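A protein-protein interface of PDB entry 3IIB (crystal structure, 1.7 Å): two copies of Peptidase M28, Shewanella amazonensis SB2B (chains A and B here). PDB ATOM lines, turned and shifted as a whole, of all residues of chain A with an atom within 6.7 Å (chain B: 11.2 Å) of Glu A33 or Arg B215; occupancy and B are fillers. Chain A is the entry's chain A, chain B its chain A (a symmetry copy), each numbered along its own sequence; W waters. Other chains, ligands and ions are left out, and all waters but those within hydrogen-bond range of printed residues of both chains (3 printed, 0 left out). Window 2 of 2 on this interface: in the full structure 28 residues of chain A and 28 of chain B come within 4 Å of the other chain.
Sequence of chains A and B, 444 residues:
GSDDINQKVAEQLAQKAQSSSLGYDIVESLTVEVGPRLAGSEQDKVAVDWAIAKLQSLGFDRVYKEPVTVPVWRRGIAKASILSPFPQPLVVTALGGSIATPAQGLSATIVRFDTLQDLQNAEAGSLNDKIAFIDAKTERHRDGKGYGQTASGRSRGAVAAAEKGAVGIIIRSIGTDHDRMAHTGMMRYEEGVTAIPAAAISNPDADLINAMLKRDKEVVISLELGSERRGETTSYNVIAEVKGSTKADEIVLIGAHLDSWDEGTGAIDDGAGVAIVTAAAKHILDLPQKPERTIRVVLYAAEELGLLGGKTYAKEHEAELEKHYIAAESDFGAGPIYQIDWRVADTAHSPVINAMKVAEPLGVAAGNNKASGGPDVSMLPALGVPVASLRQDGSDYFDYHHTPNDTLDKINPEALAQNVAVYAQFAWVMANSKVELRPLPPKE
Glu A28 touches Ala B211 (OE2 to CB, 3.7 Å).
CA of Ser A29 touches NH2 of Arg B215, 3.9 Å away.
CB of Phe B86 touches O of Val A32 (3.5 Å).
CD1 of Leu B208 touches CA of Val A32 (3.8 Å).
CB of Ala B211 touches CG2 of Val A32, at 3.7 Å.
CE of Met B212 touches O of Val A32 (3.5 Å).
Val A32 touches Arg B215 (CG1 to NH1, 3.6 Å).
Glu A33 touches Phe B86 (O to CD1, 3.5 Å).
Gln B88 touches Val A34 (NE2 to C, 3.9 Å).
Gln B88 touches Gly A35 (OE1 to CA, 3.5 Å).
NH2 of Arg B215 lies within salt-bridge range of OE1 of Glu A28 (2.8 Å).
The side-chain amide nitrogen of Gln B88 is in hydrogen-bond range of the backbone carbonyl oxygen of Thr A31 (2.8 Å).
The backbone carbonyl oxygen of Val A32 lies within hydrogen-bond range of the side-chain amide nitrogen of Gln B88, at 2.9 Å.
The side-chain carboxylate (OE2) of Glu A33 lies within salt-bridge range of the guanidinium group (NH2) of Arg B215 (2.9 Å).
Of chain B, only Ala B211 and Arg B215 come within 4 Å of Glu A28.
Ser A29 touches just one residue of chain B: Arg B215.
Printed residues of chain B within 4 Å of Thr A31: Gln B88 (2.8 Å).
Of chain B, only Phe B86 (3.5 Å), Gln B88 (2.9 Å), Leu B208 (3.8 Å), Ala B211 (3.7 Å), Met B212 (3.5 Å) and Arg B215 (3.6 Å) come within 4 Å of Val A32.
Glu A33 touches two residues of chain B.
Val A34 touches one residue of chain B.
Of the printed residues of chain B, Gly A35 touches Gln B88 (3.5 Å).
Leu B83 touches none of the printed residues of chain A.
Printed residues of chain A within 4 Å of Phe B86: Val A32 and Glu A33.
Of the printed residues of chain A, Gln B88 touches Thr A31, Val A32, Val A34 and Gly A35.
Arg B215 touches four residues of chain A.
Water W3 lies within hydrogen-bond range of O of Pro B87 (2.7 Å) and O of Val A34 (2.9 Å).
Water W2 lies within hydrogen-bond range of O of Val A34 and O of Pro B87.
Water W1 bridges the guanidinium group (NE) of Arg B215 (2.9 Å) and the side-chain carboxylate (OE2) of Glu A33 (3.5 Å).
Printed residues of chain B that touch a printed residue of chain A: Phe B86, Gln B88, Leu B208, Ala B211, Met B212 and Arg B215.
Of the 12 printed residues of chain A, 7 touch a printed residue of chain B.
Hydrophobic or aromatic side chains of chain A that line the printed part of chain B: Val A32.
No position is printed for both chains.
Of the 14 pairs that touch across the chains among the printed residues, none has its exchanged pair printed and touching as well.
The backbone carbonyl oxygen (O) of Glu A28 sits at hydrogen-bond distance from the side-chain hydroxyl (OG1) of Thr A31.
The indole nitrogen (NE1) of Trp A50 sits at hydrogen-bond distance from the side-chain hydroxyl (OG) of Ser A29 (2.9 Å).
The side-chain hydroxyl (OG) of Ser A29 is in hydrogen-bond range of the side-chain amino group (NZ) of Lys A54, 3.2 Å away.
O of Leu A30 lies within hydrogen-bond range of N of Gly A35 (3.0 Å).
O of Gln B88 is in hydrogen-bond range of N of Ile B82 (2.7 Å).
The backbone carbonyl oxygen of Ala B211 sits at hydrogen-bond distance from the guanidinium group of Arg B215.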
ATOM      1  N   ASP A  25      -9.356  16.427  14.259  1.00  0.00           N
ATOM      2  CA  ASP A  25      -9.852  17.689  14.813  1.00  0.00           C
ATOM      3  C   ASP A  25     -11.013  18.255  13.997  1.00  0.00           C
ATOM      4  O   ASP A  25     -11.911  18.856  14.559  1.00  0.00           O
ATOM      5  CB  ASP A  25      -8.734  18.732  14.858  1.00  0.00           C
ATOM      6  CG  ASP A  25      -7.630  18.406  15.863  1.00  0.00           C
ATOM      7  OD1 ASP A  25      -7.841  17.647  16.826  1.00  0.00           O
ATOM      8  OD2 ASP A  25      -6.527  18.926  15.632  1.00  0.00           O
ATOM      9  N   GLU A  28     -14.042  16.074  14.880  1.00  0.00           N
ATOM     10  CA  GLU A  28     -14.435  16.389  16.269  1.00  0.00           C
ATOM     11  C   GLU A  28     -15.208  17.718  16.251  1.00  0.00           C
ATOM     12  O   GLU A  28     -16.244  17.845  16.876  1.00  0.00           O
ATOM     13  CB  GLU A  28     -13.226  16.485  17.178  1.00  0.00           C
ATOM     14  CG  GLU A  28     -13.531  16.594  18.661  1.00  0.00           C
ATOM     15  CD  GLU A  28     -13.777  18.028  19.153  1.00  0.00           C
ATOM     16  OE1 GLU A  28     -13.629  19.006  18.399  1.00  0.00           O
ATOM     17  OE2 GLU A  28     -14.124  18.162  20.346  1.00  0.00           O
ATOM     18  N   SER A  29     -14.700  18.673  15.474  1.00  0.00           N
ATOM     19  CA  SER A  29     -15.328  19.989  15.414  1.00  0.00           C
ATOM     20  C   SER A  29     -16.758  19.920  14.870  1.00  0.00           C
ATOM     21  O   SER A  29     -17.696  20.523  15.416  1.00  0.00           O
ATOM     22  CB  SER A  29     -14.444  20.907  14.600  1.00  0.00           C
ATOM     23  OG  SER A  29     -15.047  22.200  14.484  1.00  0.00           O
ATOM     24  N   LEU A  30     -16.916  19.154  13.793  1.00  0.00           N
ATOM     25  CA  LEU A  30     -18.194  19.057  13.112  1.00  0.00           C
ATOM     26  C   LEU A  30     -19.211  18.350  14.013  1.00  0.00           C
ATOM     27  O   LEU A  30     -20.352  18.819  14.215  1.00  0.00           O
ATOM     28  CB  LEU A  30     -18.022  18.304  11.777  1.00  0.00           C
ATOM     29  CG  LEU A  30     -19.276  18.015  10.921  1.00  0.00           C
ATOM     30  CD1 LEU A  30     -20.145  19.244  10.624  1.00  0.00           C
ATOM     31  CD2 LEU A  30     -18.861  17.277   9.619  1.00  0.00           C
ATOM     32  N   THR A  31     -18.793  17.220  14.578  1.00  0.00           N
ATOM     33  CA  THR A  31     -19.726  16.413  15.379  1.00  0.00           C
ATOM     34  C   THR A  31     -20.103  17.113  16.688  1.00  0.00           C
ATOM     35  O   THR A  31     -21.239  16.972  17.153  1.00  0.00           O
ATOM     36  CB  THR A  31     -19.209  14.986  15.652  1.00  0.00           C
ATOM     37  OG1 THR A  31     -17.933  15.063  16.296  1.00  0.00           O
ATOM     38  CG2 THR A  31     -19.080  14.186  14.347  1.00  0.00           C
ATOM     39  N   VAL A  32     -19.191  17.891  17.272  1.00  0.00           N
ATOM     40  CA  VAL A  32     -19.498  18.631  18.516  1.00  0.00           C
ATOM     41  C   VAL A  32     -20.243  19.943  18.263  1.00  0.00           C
ATOM     42  O   VAL A  32     -21.259  20.207  18.912  1.00  0.00           O
ATOM     43  CB  VAL A  32     -18.220  18.915  19.327  1.00  0.00           C
ATOM     44  CG1 VAL A  32     -18.530  19.815  20.580  1.00  0.00           C
ATOM     45  CG2 VAL A  32     -17.534  17.592  19.715  1.00  0.00           C
ATOM     46  N   GLU A  33     -19.768  20.739  17.293  1.00  0.00           N
ATOM     47  CA  GLU A  33     -20.280  22.104  17.106  1.00  0.00           C
ATOM     48  C   GLU A  33     -21.547  22.191  16.211  1.00  0.00           C
ATOM     49  O   GLU A  33     -22.194  23.235  16.166  1.00  0.00           O
ATOM     50  CB  GLU A  33     -19.182  22.996  16.556  1.00  0.00           C
ATOM     51  CG  GLU A  33     -17.901  23.059  17.425  1.00  0.00           C
ATOM     52  CD  GLU A  33     -16.738  23.683  16.686  1.00  0.00           C
ATOM     53  OE1 GLU A  33     -17.004  24.549  15.838  1.00  0.00           O
ATOM     54  OE2 GLU A  33     -15.562  23.251  16.860  1.00  0.00           O
ATOM     55  N   VAL A  34     -21.851  21.097  15.525  1.00  0.00           N
ATOM     56  CA  VAL A  34     -23.047  20.945  14.722  1.00  0.00           C
ATOM     57  C   VAL A  34     -23.825  19.742  15.146  1.00  0.00           C
ATOM     58  O   VAL A  34     -25.007  19.880  15.455  1.00  0.00           O
ATOM     59  CB  VAL A  34     -22.708  20.853  13.208  1.00  0.00           C
ATOM     60  CG1 VAL A  34     -23.982  20.859  12.337  1.00  0.00           C
ATOM     61  CG2 VAL A  34     -21.789  22.006  12.810  1.00  0.00           C
ATOM     62  N   GLY A  35     -23.216  18.555  15.124  1.00  0.00           N
ATOM     63  CA  GLY A  35     -23.954  17.332  15.369  1.00  0.00           C
ATOM     64  C   GLY A  35     -24.701  16.860  14.121  1.00  0.00           C
ATOM     65  O   GLY A  35     -24.293  17.160  12.992  1.00  0.00           O
ATOM     66  N   VAL A  46     -26.733  25.426   9.990  1.00  0.00           N
ATOM     67  CA  VAL A  46     -25.633  25.355  10.990  1.00  0.00           C
ATOM     68  C   VAL A  46     -24.398  24.664  10.434  1.00  0.00           C
ATOM     69  O   VAL A  46     -23.294  25.180  10.607  1.00  0.00           O
ATOM     70  CB  VAL A  46     -26.095  24.745  12.341  1.00  0.00           C
ATOM     71  CG1 VAL A  46     -24.940  24.617  13.351  1.00  0.00           C
ATOM     72  CG2 VAL A  46     -27.312  25.590  12.928  1.00  0.00           C
ATOM     73  N   TRP A  50     -20.850  26.386   9.533  1.00  0.00           N
ATOM     74  CA  TRP A  50     -19.673  25.803  10.192  1.00  0.00           C
ATOM     75  C   TRP A  50     -18.582  25.531   9.151  1.00  0.00           C
ATOM     76  O   TRP A  50     -17.418  25.808   9.396  1.00  0.00           O
ATOM     77  CB  TRP A  50     -20.042  24.528  10.948  1.00  0.00           C
ATOM     78  CG  TRP A  50     -18.830  23.704  11.337  1.00  0.00           C
ATOM     79  CD1 TRP A  50     -18.153  23.767  12.509  1.00  0.00           C
ATOM     80  CD2 TRP A  50     -18.167  22.728  10.534  1.00  0.00           C
ATOM     81  NE1 TRP A  50     -17.092  22.892  12.492  1.00  0.00           N
ATOM     82  CE2 TRP A  50     -17.094  22.221  11.294  1.00  0.00           C
ATOM     83  CE3 TRP A  50     -18.408  22.186   9.251  1.00  0.00           C
ATOM     84  CZ2 TRP A  50     -16.227  21.241  10.804  1.00  0.00           C
ATOM     85  CZ3 TRP A  50     -17.532  21.208   8.758  1.00  0.00           C
ATOM     86  CH2 TRP A  50     -16.449  20.746   9.541  1.00  0.00           C
ATOM     87  N   LYS A  54     -14.941  27.107   8.765  1.00  0.00           N
ATOM     88  CA  LYS A  54     -13.826  26.203   8.926  1.00  0.00           C
ATOM     89  C   LYS A  54     -12.883  26.327   7.781  1.00  0.00           C
ATOM     90  O   LYS A  54     -11.663  26.393   7.968  1.00  0.00           O
ATOM     91  CB  LYS A  54     -14.316  24.760   9.091  1.00  0.00           C
ATOM     92  CG  LYS A  54     -13.203  23.731   9.336  1.00  0.00           C
ATOM     93  CD  LYS A  54     -12.529  23.952  10.699  1.00  0.00           C
ATOM     94  CE  LYS A  54     -13.482  23.811  11.885  1.00  0.00           C
ATOM     95  NZ  LYS A  54     -12.773  23.980  13.197  1.00  0.00           N
ATOM     96  N   ILE B  82     -29.207  18.859  24.479  1.00  0.00           N
ATOM     97  CA  ILE B  82     -28.406  20.031  24.819  1.00  0.00           C
ATOM     98  C   ILE B  82     -29.021  21.221  24.114  1.00  0.00           C
ATOM     99  O   ILE B  82     -29.303  21.174  22.901  1.00  0.00           O
ATOM    100  CB  ILE B  82     -26.979  19.828  24.355  1.00  0.00           C
ATOM    101  CG1 ILE B  82     -26.314  18.719  25.192  1.00  0.00           C
ATOM    102  CG2 ILE B  82     -26.216  21.112  24.472  1.00  0.00           C
ATOM    103  CD1 ILE B  82     -24.945  18.326  24.489  1.00  0.00           C
ATOM    104  N   LEU B  83     -29.264  22.281  24.877  1.00  0.00           N
ATOM    105  CA  LEU B  83     -29.848  23.524  24.336  1.00  0.00           C
ATOM    106  C   LEU B  83     -28.787  24.521  23.902  1.00  0.00           C
ATOM    107  O   LEU B  83     -28.998  25.277  22.937  1.00  0.00           O
ATOM    108  CB  LEU B  83     -30.797  24.182  25.352  1.00  0.00           C
ATOM    109  CG  LEU B  83     -31.998  23.352  25.825  1.00  0.00           C
ATOM    110  CD1 LEU B  83     -32.804  24.158  26.874  1.00  0.00           C
ATOM    111  CD2 LEU B  83     -32.897  22.954  24.682  1.00  0.00           C
ATOM    112  N   SER B  84     -27.662  24.508  24.606  1.00  0.00           N
ATOM    113  CA  SER B  84     -26.549  25.391  24.320  1.00  0.00           C
ATOM    114  C   SER B  84     -25.280  24.835  24.967  1.00  0.00           C
ATOM    115  O   SER B  84     -25.341  24.144  25.974  1.00  0.00           O
ATOM    116  CB  SER B  84     -26.844  26.826  24.794  1.00  0.00           C
ATOM    117  OG  SER B  84     -27.014  26.868  26.186  1.00  0.00           O
ATOM    118  N   PRO B  85     -24.100  25.133  24.368  1.00  0.00           N
ATOM    119  CA  PRO B  85     -23.822  26.045  23.231  1.00  0.00           C
ATOM    120  C   PRO B  85     -24.258  25.558  21.817  1.00  0.00           C
ATOM    121  O   PRO B  85     -24.573  26.373  20.968  1.00  0.00           O
ATOM    122  CB  PRO B  85     -22.318  26.184  23.286  1.00  0.00           C
ATOM    123  CG  PRO B  85     -21.828  24.902  23.918  1.00  0.00           C
ATOM    124  CD  PRO B  85     -22.882  24.487  24.867  1.00  0.00           C
ATOM    125  N   PHE B  86     -24.248  24.245  21.587  1.00  0.00           N
ATOM    126  CA  PHE B  86     -24.506  23.671  20.277  1.00  0.00           C
ATOM    127  C   PHE B  86     -25.659  22.695  20.448  1.00  0.00           C
ATOM    128  O   PHE B  86     -25.481  21.623  21.063  1.00  0.00           O
ATOM    129  CB  PHE B  86     -23.274  22.906  19.787  1.00  0.00           C
ATOM    130  CG  PHE B  86     -22.000  23.698  19.897  1.00  0.00           C
ATOM    131  CD1 PHE B  86     -21.855  24.895  19.197  1.00  0.00           C
ATOM    132  CD2 PHE B  86     -20.973  23.285  20.738  1.00  0.00           C
ATOM    133  CE1 PHE B  86     -20.714  25.631  19.312  1.00  0.00           C
ATOM    134  CE2 PHE B  86     -19.821  24.024  20.831  1.00  0.00           C
ATOM    135  CZ  PHE B  86     -19.696  25.191  20.141  1.00  0.00           C
ATOM    136  N   PRO B  87     -26.837  23.049  19.912  1.00  0.00           N
ATOM    137  CA  PRO B  87     -27.970  22.220  20.251  1.00  0.00           C
ATOM    138  C   PRO B  87     -27.850  20.824  19.644  1.00  0.00           C
ATOM    139  O   PRO B  87     -27.575  20.695  18.463  1.00  0.00           O
ATOM    140  CB  PRO B  87     -29.145  22.980  19.633  1.00  0.00           C
ATOM    141  CG  PRO B  87     -28.695  24.351  19.503  1.00  0.00           C
ATOM    142  CD  PRO B  87     -27.255  24.287  19.220  1.00  0.00           C
ATOM    143  N   GLN B  88     -28.115  19.798  20.433  1.00  0.00           N
ATOM    144  CA  GLN B  88     -28.028  18.432  19.981  1.00  0.00           C
ATOM    145  C   GLN B  88     -28.903  17.505  20.812  1.00  0.00           C
ATOM    146  O   GLN B  88     -29.064  17.722  22.013  1.00  0.00           O
ATOM    147  CB  GLN B  88     -26.601  17.934  20.153  1.00  0.00           C
ATOM    148  CG  GLN B  88     -25.599  18.572  19.277  1.00  0.00           C
ATOM    149  CD  GLN B  88     -24.496  17.663  18.879  1.00  0.00           C
ATOM    150  OE1 GLN B  88     -24.720  16.499  18.659  1.00  0.00           O
ATOM    151  NE2 GLN B  88     -23.288  18.219  18.671  1.00  0.00           N
ATOM    152  N   PRO B  89     -29.349  16.392  20.219  1.00  0.00           N
ATOM    153  CA  PRO B  89     -30.070  15.345  20.963  1.00  0.00           C
ATOM    154  C   PRO B  89     -29.166  14.570  21.910  1.00  0.00           C
ATOM    155  O   PRO B  89     -27.958  14.423  21.655  1.00  0.00           O
ATOM    156  CB  PRO B  89     -30.560  14.391  19.860  1.00  0.00           C
ATOM    157  CG  PRO B  89     -30.400  15.122  18.578  1.00  0.00           C
ATOM    158  CD  PRO B  89     -29.259  16.057  18.791  1.00  0.00           C
ATOM    159  N   ARG B 112     -20.435  19.930  36.127  1.00  0.00           N
ATOM    160  CA  ARG B 112     -19.800  18.641  35.992  1.00  0.00           C
ATOM    161  C   ARG B 112     -18.955  18.291  37.219  1.00  0.00           C
ATOM    162  O   ARG B 112     -18.227  19.127  37.737  1.00  0.00           O
ATOM    163  CB  ARG B 112     -18.886  18.630  34.752  1.00  0.00           C
ATOM    164  CG  ARG B 112     -18.210  17.294  34.497  1.00  0.00           C
ATOM    165  CD  ARG B 112     -17.184  17.381  33.349  1.00  0.00           C
ATOM    166  NE  ARG B 112     -16.422  16.133  33.281  1.00  0.00           N
ATOM    167  CZ  ARG B 112     -15.507  15.750  34.179  1.00  0.00           C
ATOM    168  NH1 ARG B 112     -15.142  16.562  35.166  1.00  0.00           N
ATOM    169  NH2 ARG B 112     -14.900  14.567  34.065  1.00  0.00           N
ATOM    170  N   ALA B 206     -22.086  11.746  27.109  1.00  0.00           N
ATOM    171  CA  ALA B 206     -21.283  12.297  28.191  1.00  0.00           C
ATOM    172  C   ALA B 206     -19.958  12.829  27.587  1.00  0.00           C
ATOM    173  O   ALA B 206     -19.500  13.917  27.962  1.00  0.00           O
ATOM    174  CB  ALA B 206     -21.019  11.228  29.236  1.00  0.00           C
ATOM    175  N   ASP B 207     -19.404  12.091  26.598  1.00  0.00           N
ATOM    176  CA  ASP B 207     -18.209  12.554  25.891  1.00  0.00           C
ATOM    177  C   ASP B 207     -18.526  13.899  25.192  1.00  0.00           C
ATOM    178  O   ASP B 207     -17.703  14.801  25.161  1.00  0.00           O
ATOM    179  CB  ASP B 207     -17.748  11.595  24.803  1.00  0.00           C
ATOM    180  CG  ASP B 207     -17.257  10.286  25.334  1.00  0.00           C
ATOM    181  OD1 ASP B 207     -16.940  10.211  26.550  1.00  0.00           O
ATOM    182  OD2 ASP B 207     -17.231   9.318  24.536  1.00  0.00           O
ATOM    183  N   LEU B 208     -19.711  13.991  24.594  1.00  0.00           N
ATOM    184  CA  LEU B 208     -20.102  15.199  23.866  1.00  0.00           C
ATOM    185  C   LEU B 208     -20.191  16.407  24.800  1.00  0.00           C
ATOM    186  O   LEU B 208     -19.729  17.510  24.470  1.00  0.00           O
ATOM    187  CB  LEU B 208     -21.435  14.985  23.149  1.00  0.00           C
ATOM    188  CG  LEU B 208     -22.068  16.184  22.441  1.00  0.00           C
ATOM    189  CD1 LEU B 208     -21.141  16.649  21.318  1.00  0.00           C
ATOM    190  CD2 LEU B 208     -23.470  15.736  21.902  1.00  0.00           C
ATOM    191  N   ILE B 209     -20.795  16.197  25.962  1.00  0.00           N
ATOM    192  CA  ILE B 209     -20.977  17.262  26.911  1.00  0.00           C
ATOM    193  C   ILE B 209     -19.558  17.718  27.337  1.00  0.00           C
ATOM    194  O   ILE B 209     -19.274  18.907  27.423  1.00  0.00           O
ATOM    195  CB  ILE B 209     -21.795  16.830  28.112  1.00  0.00           C
ATOM    196  CG1 ILE B 209     -23.259  16.659  27.721  1.00  0.00           C
ATOM    197  CG2 ILE B 209     -21.690  17.882  29.235  1.00  0.00           C
ATOM    198  CD1 ILE B 209     -24.220  16.250  28.894  1.00  0.00           C
ATOM    199  N   ASN B 210     -18.679  16.760  27.589  1.00  0.00           N
ATOM    200  CA  ASN B 210     -17.301  17.068  27.984  1.00  0.00           C
ATOM    201  C   ASN B 210     -16.598  17.935  26.926  1.00  0.00           C
ATOM    202  O   ASN B 210     -15.923  18.905  27.271  1.00  0.00           O
ATOM    203  CB  ASN B 210     -16.473  15.800  28.200  1.00  0.00           C
ATOM    204  CG  ASN B 210     -16.699  15.140  29.570  1.00  0.00           C
ATOM    205  OD1 ASN B 210     -17.184  15.757  30.534  1.00  0.00           O
ATOM    206  ND2 ASN B 210     -16.263  13.879  29.671  1.00  0.00           N
ATOM    207  N   ALA B 211     -16.747  17.585  25.648  1.00  0.00           N
ATOM    208  CA  ALA B 211     -16.129  18.328  24.529  1.00  0.00           C
ATOM    209  C   ALA B 211     -16.588  19.792  24.480  1.00  0.00           C
ATOM    210  O   ALA B 211     -15.817  20.696  24.145  1.00  0.00           O
ATOM    211  CB  ALA B 211     -16.475  17.629  23.214  1.00  0.00           C
ATOM    212  N   MET B 212     -17.857  20.029  24.809  1.00  0.00           N
ATOM    213  CA  MET B 212     -18.359  21.396  24.915  1.00  0.00           C
ATOM    214  C   MET B 212     -17.808  22.168  26.128  1.00  0.00           C
ATOM    215  O   MET B 212     -17.493  23.355  26.010  1.00  0.00           O
ATOM    216  CB  MET B 212     -19.883  21.356  24.967  1.00  0.00           C
ATOM    217  CG  MET B 212     -20.488  21.010  23.621  1.00  0.00           C
ATOM    218  SD  MET B 212     -22.401  21.122  23.613  1.00  0.00           S
ATOM    219  CE  MET B 212     -22.726  19.926  22.082  1.00  0.00           C
ATOM    220  N   LEU B 213     -17.748  21.498  27.294  1.00  0.00           N
ATOM    221  CA  LEU B 213     -17.181  22.054  28.501  1.00  0.00           C
ATOM    222  C   LEU B 213     -15.717  22.375  28.313  1.00  0.00           C
ATOM    223  O   LEU B 213     -15.238  23.377  28.834  1.00  0.00           O
ATOM    224  CB  LEU B 213     -17.362  21.109  29.686  1.00  0.00           C
ATOM    225  CG  LEU B 213     -18.819  20.897  30.135  1.00  0.00           C
ATOM    226  CD1 LEU B 213     -18.857  19.719  31.143  1.00  0.00           C
ATOM    227  CD2 LEU B 213     -19.447  22.168  30.715  1.00  0.00           C
ATOM    228  N   LYS B 214     -15.012  21.534  27.560  1.00  0.00           N
ATOM    229  CA  LYS B 214     -13.587  21.755  27.279  1.00  0.00           C
ATOM    230  C   LYS B 214     -13.368  22.993  26.425  1.00  0.00           C
ATOM    231  O   LYS B 214     -12.246  23.494  26.363  1.00  0.00           O
ATOM    232  CB  LYS B 214     -12.925  20.542  26.588  1.00  0.00           C
ATOM    233  CG  LYS B 214     -12.564  19.403  27.522  1.00  0.00           C
ATOM    234  CD  LYS B 214     -11.658  18.371  26.850  1.00  0.00           C
ATOM    235  N   ARG B 215     -14.421  23.484  25.775  1.00  0.00           N
ATOM    236  CA  ARG B 215     -14.351  24.724  25.030  1.00  0.00           C
ATOM    237  C   ARG B 215     -14.632  25.948  25.913  1.00  0.00           C
ATOM    238  O   ARG B 215     -14.792  27.057  25.394  1.00  0.00           O
ATOM    239  CB  ARG B 215     -15.340  24.691  23.867  1.00  0.00           C
ATOM    240  CG  ARG B 215     -14.870  23.798  22.725  1.00  0.00           C
ATOM    241  CD  ARG B 215     -16.081  23.362  21.868  1.00  0.00           C
ATOM    242  NE  ARG B 215     -15.720  22.894  20.535  1.00  0.00           N
ATOM    243  CZ  ARG B 215     -15.230  21.686  20.247  1.00  0.00           C
ATOM    244  NH1 ARG B 215     -15.071  20.747  21.174  1.00  0.00           N
ATOM    245  NH2 ARG B 215     -14.970  21.386  18.995  1.00  0.00           N
ATOM    246  N   ASP B 216     -14.655  25.743  27.237  1.00  0.00           N
ATOM    247  CA  ASP B 216     -14.902  26.819  28.194  1.00  0.00           C
ATOM    248  C   ASP B 216     -16.281  27.430  27.949  1.00  0.00           C
ATOM    249  O   ASP B 216     -16.473  28.628  28.071  1.00  0.00           O
ATOM    250  CB  ASP B 216     -13.782  27.871  28.152  1.00  0.00           C
ATOM    251  CG  ASP B 216     -12.414  27.287  28.476  1.00  0.00           C
ATOM    252  OD1 ASP B 216     -12.319  26.451  29.399  1.00  0.00           O
ATOM    253  OD2 ASP B 216     -11.426  27.675  27.806  1.00  0.00           O
ATOM    254  N   LYS B 217     -17.235  26.570  27.600  1.00  0.00           N
ATOM    255  CA  LYS B 217     -18.623  26.951  27.452  1.00  0.00           C
ATOM    256  C   LYS B 217     -19.419  26.305  28.588  1.00  0.00           C
ATOM    257  O   LYS B 217     -19.127  25.191  29.003  1.00  0.00           O
ATOM    258  CB  LYS B 217     -19.175  26.489  26.112  1.00  0.00           C
ATOM    259  CG  LYS B 217     -18.531  27.133  24.906  1.00  0.00           C
ATOM    260  CD  LYS B 217     -18.701  28.644  24.913  1.00  0.00           C
ATOM    261  CE  LYS B 217     -17.571  29.345  24.144  1.00  0.00           C
ATOM    262  NZ  LYS B 217     -17.682  29.108  22.691  1.00  0.00           N
ATOM    263  N   GLU B 218     -20.415  27.024  29.096  1.00  0.00           N
ATOM    264  CA  GLU B 218     -21.455  26.385  29.912  1.00  0.00           C
ATOM    265  C   GLU B 218     -22.444  25.611  29.039  1.00  0.00           C
ATOM    266  O   GLU B 218     -22.801  26.060  27.949  1.00  0.00           O
ATOM    267  CB  GLU B 218     -22.197  27.427  30.745  1.00  0.00           C
ATOM    268  CG  GLU B 218     -21.260  28.028  31.805  1.00  0.00           C
ATOM    269  CD  GLU B 218     -21.971  28.863  32.836  1.00  0.00           C
ATOM    270  OE1 GLU B 218     -22.947  29.550  32.483  1.00  0.00           O
ATOM    271  OE2 GLU B 218     -21.542  28.826  33.998  1.00  0.00           O
ATOM    272  N   VAL B 219     -22.877  24.459  29.538  1.00  0.00           N
ATOM    273  CA  VAL B 219     -23.840  23.600  28.853  1.00  0.00           C
ATOM    274  C   VAL B 219     -25.158  23.665  29.595  1.00  0.00           C
ATOM    275  O   VAL B 219     -25.224  23.568  30.853  1.00  0.00           O
ATOM    276  CB  VAL B 219     -23.329  22.148  28.782  1.00  0.00           C
ATOM    277  CG1 VAL B 219     -24.397  21.172  28.183  1.00  0.00           C
ATOM    278  CG2 VAL B 219     -21.992  22.123  28.028  1.00  0.00           C
HETATM  279  O   HOH W   1     -16.084  25.517  19.458  1.00  0.00           O
HETATM  280  O   HOH W   2     -27.503  18.851  15.935  1.00  0.00           O
HETATM  281  O   HOH W   3     -26.384  22.171  16.484  1.00  0.00           O
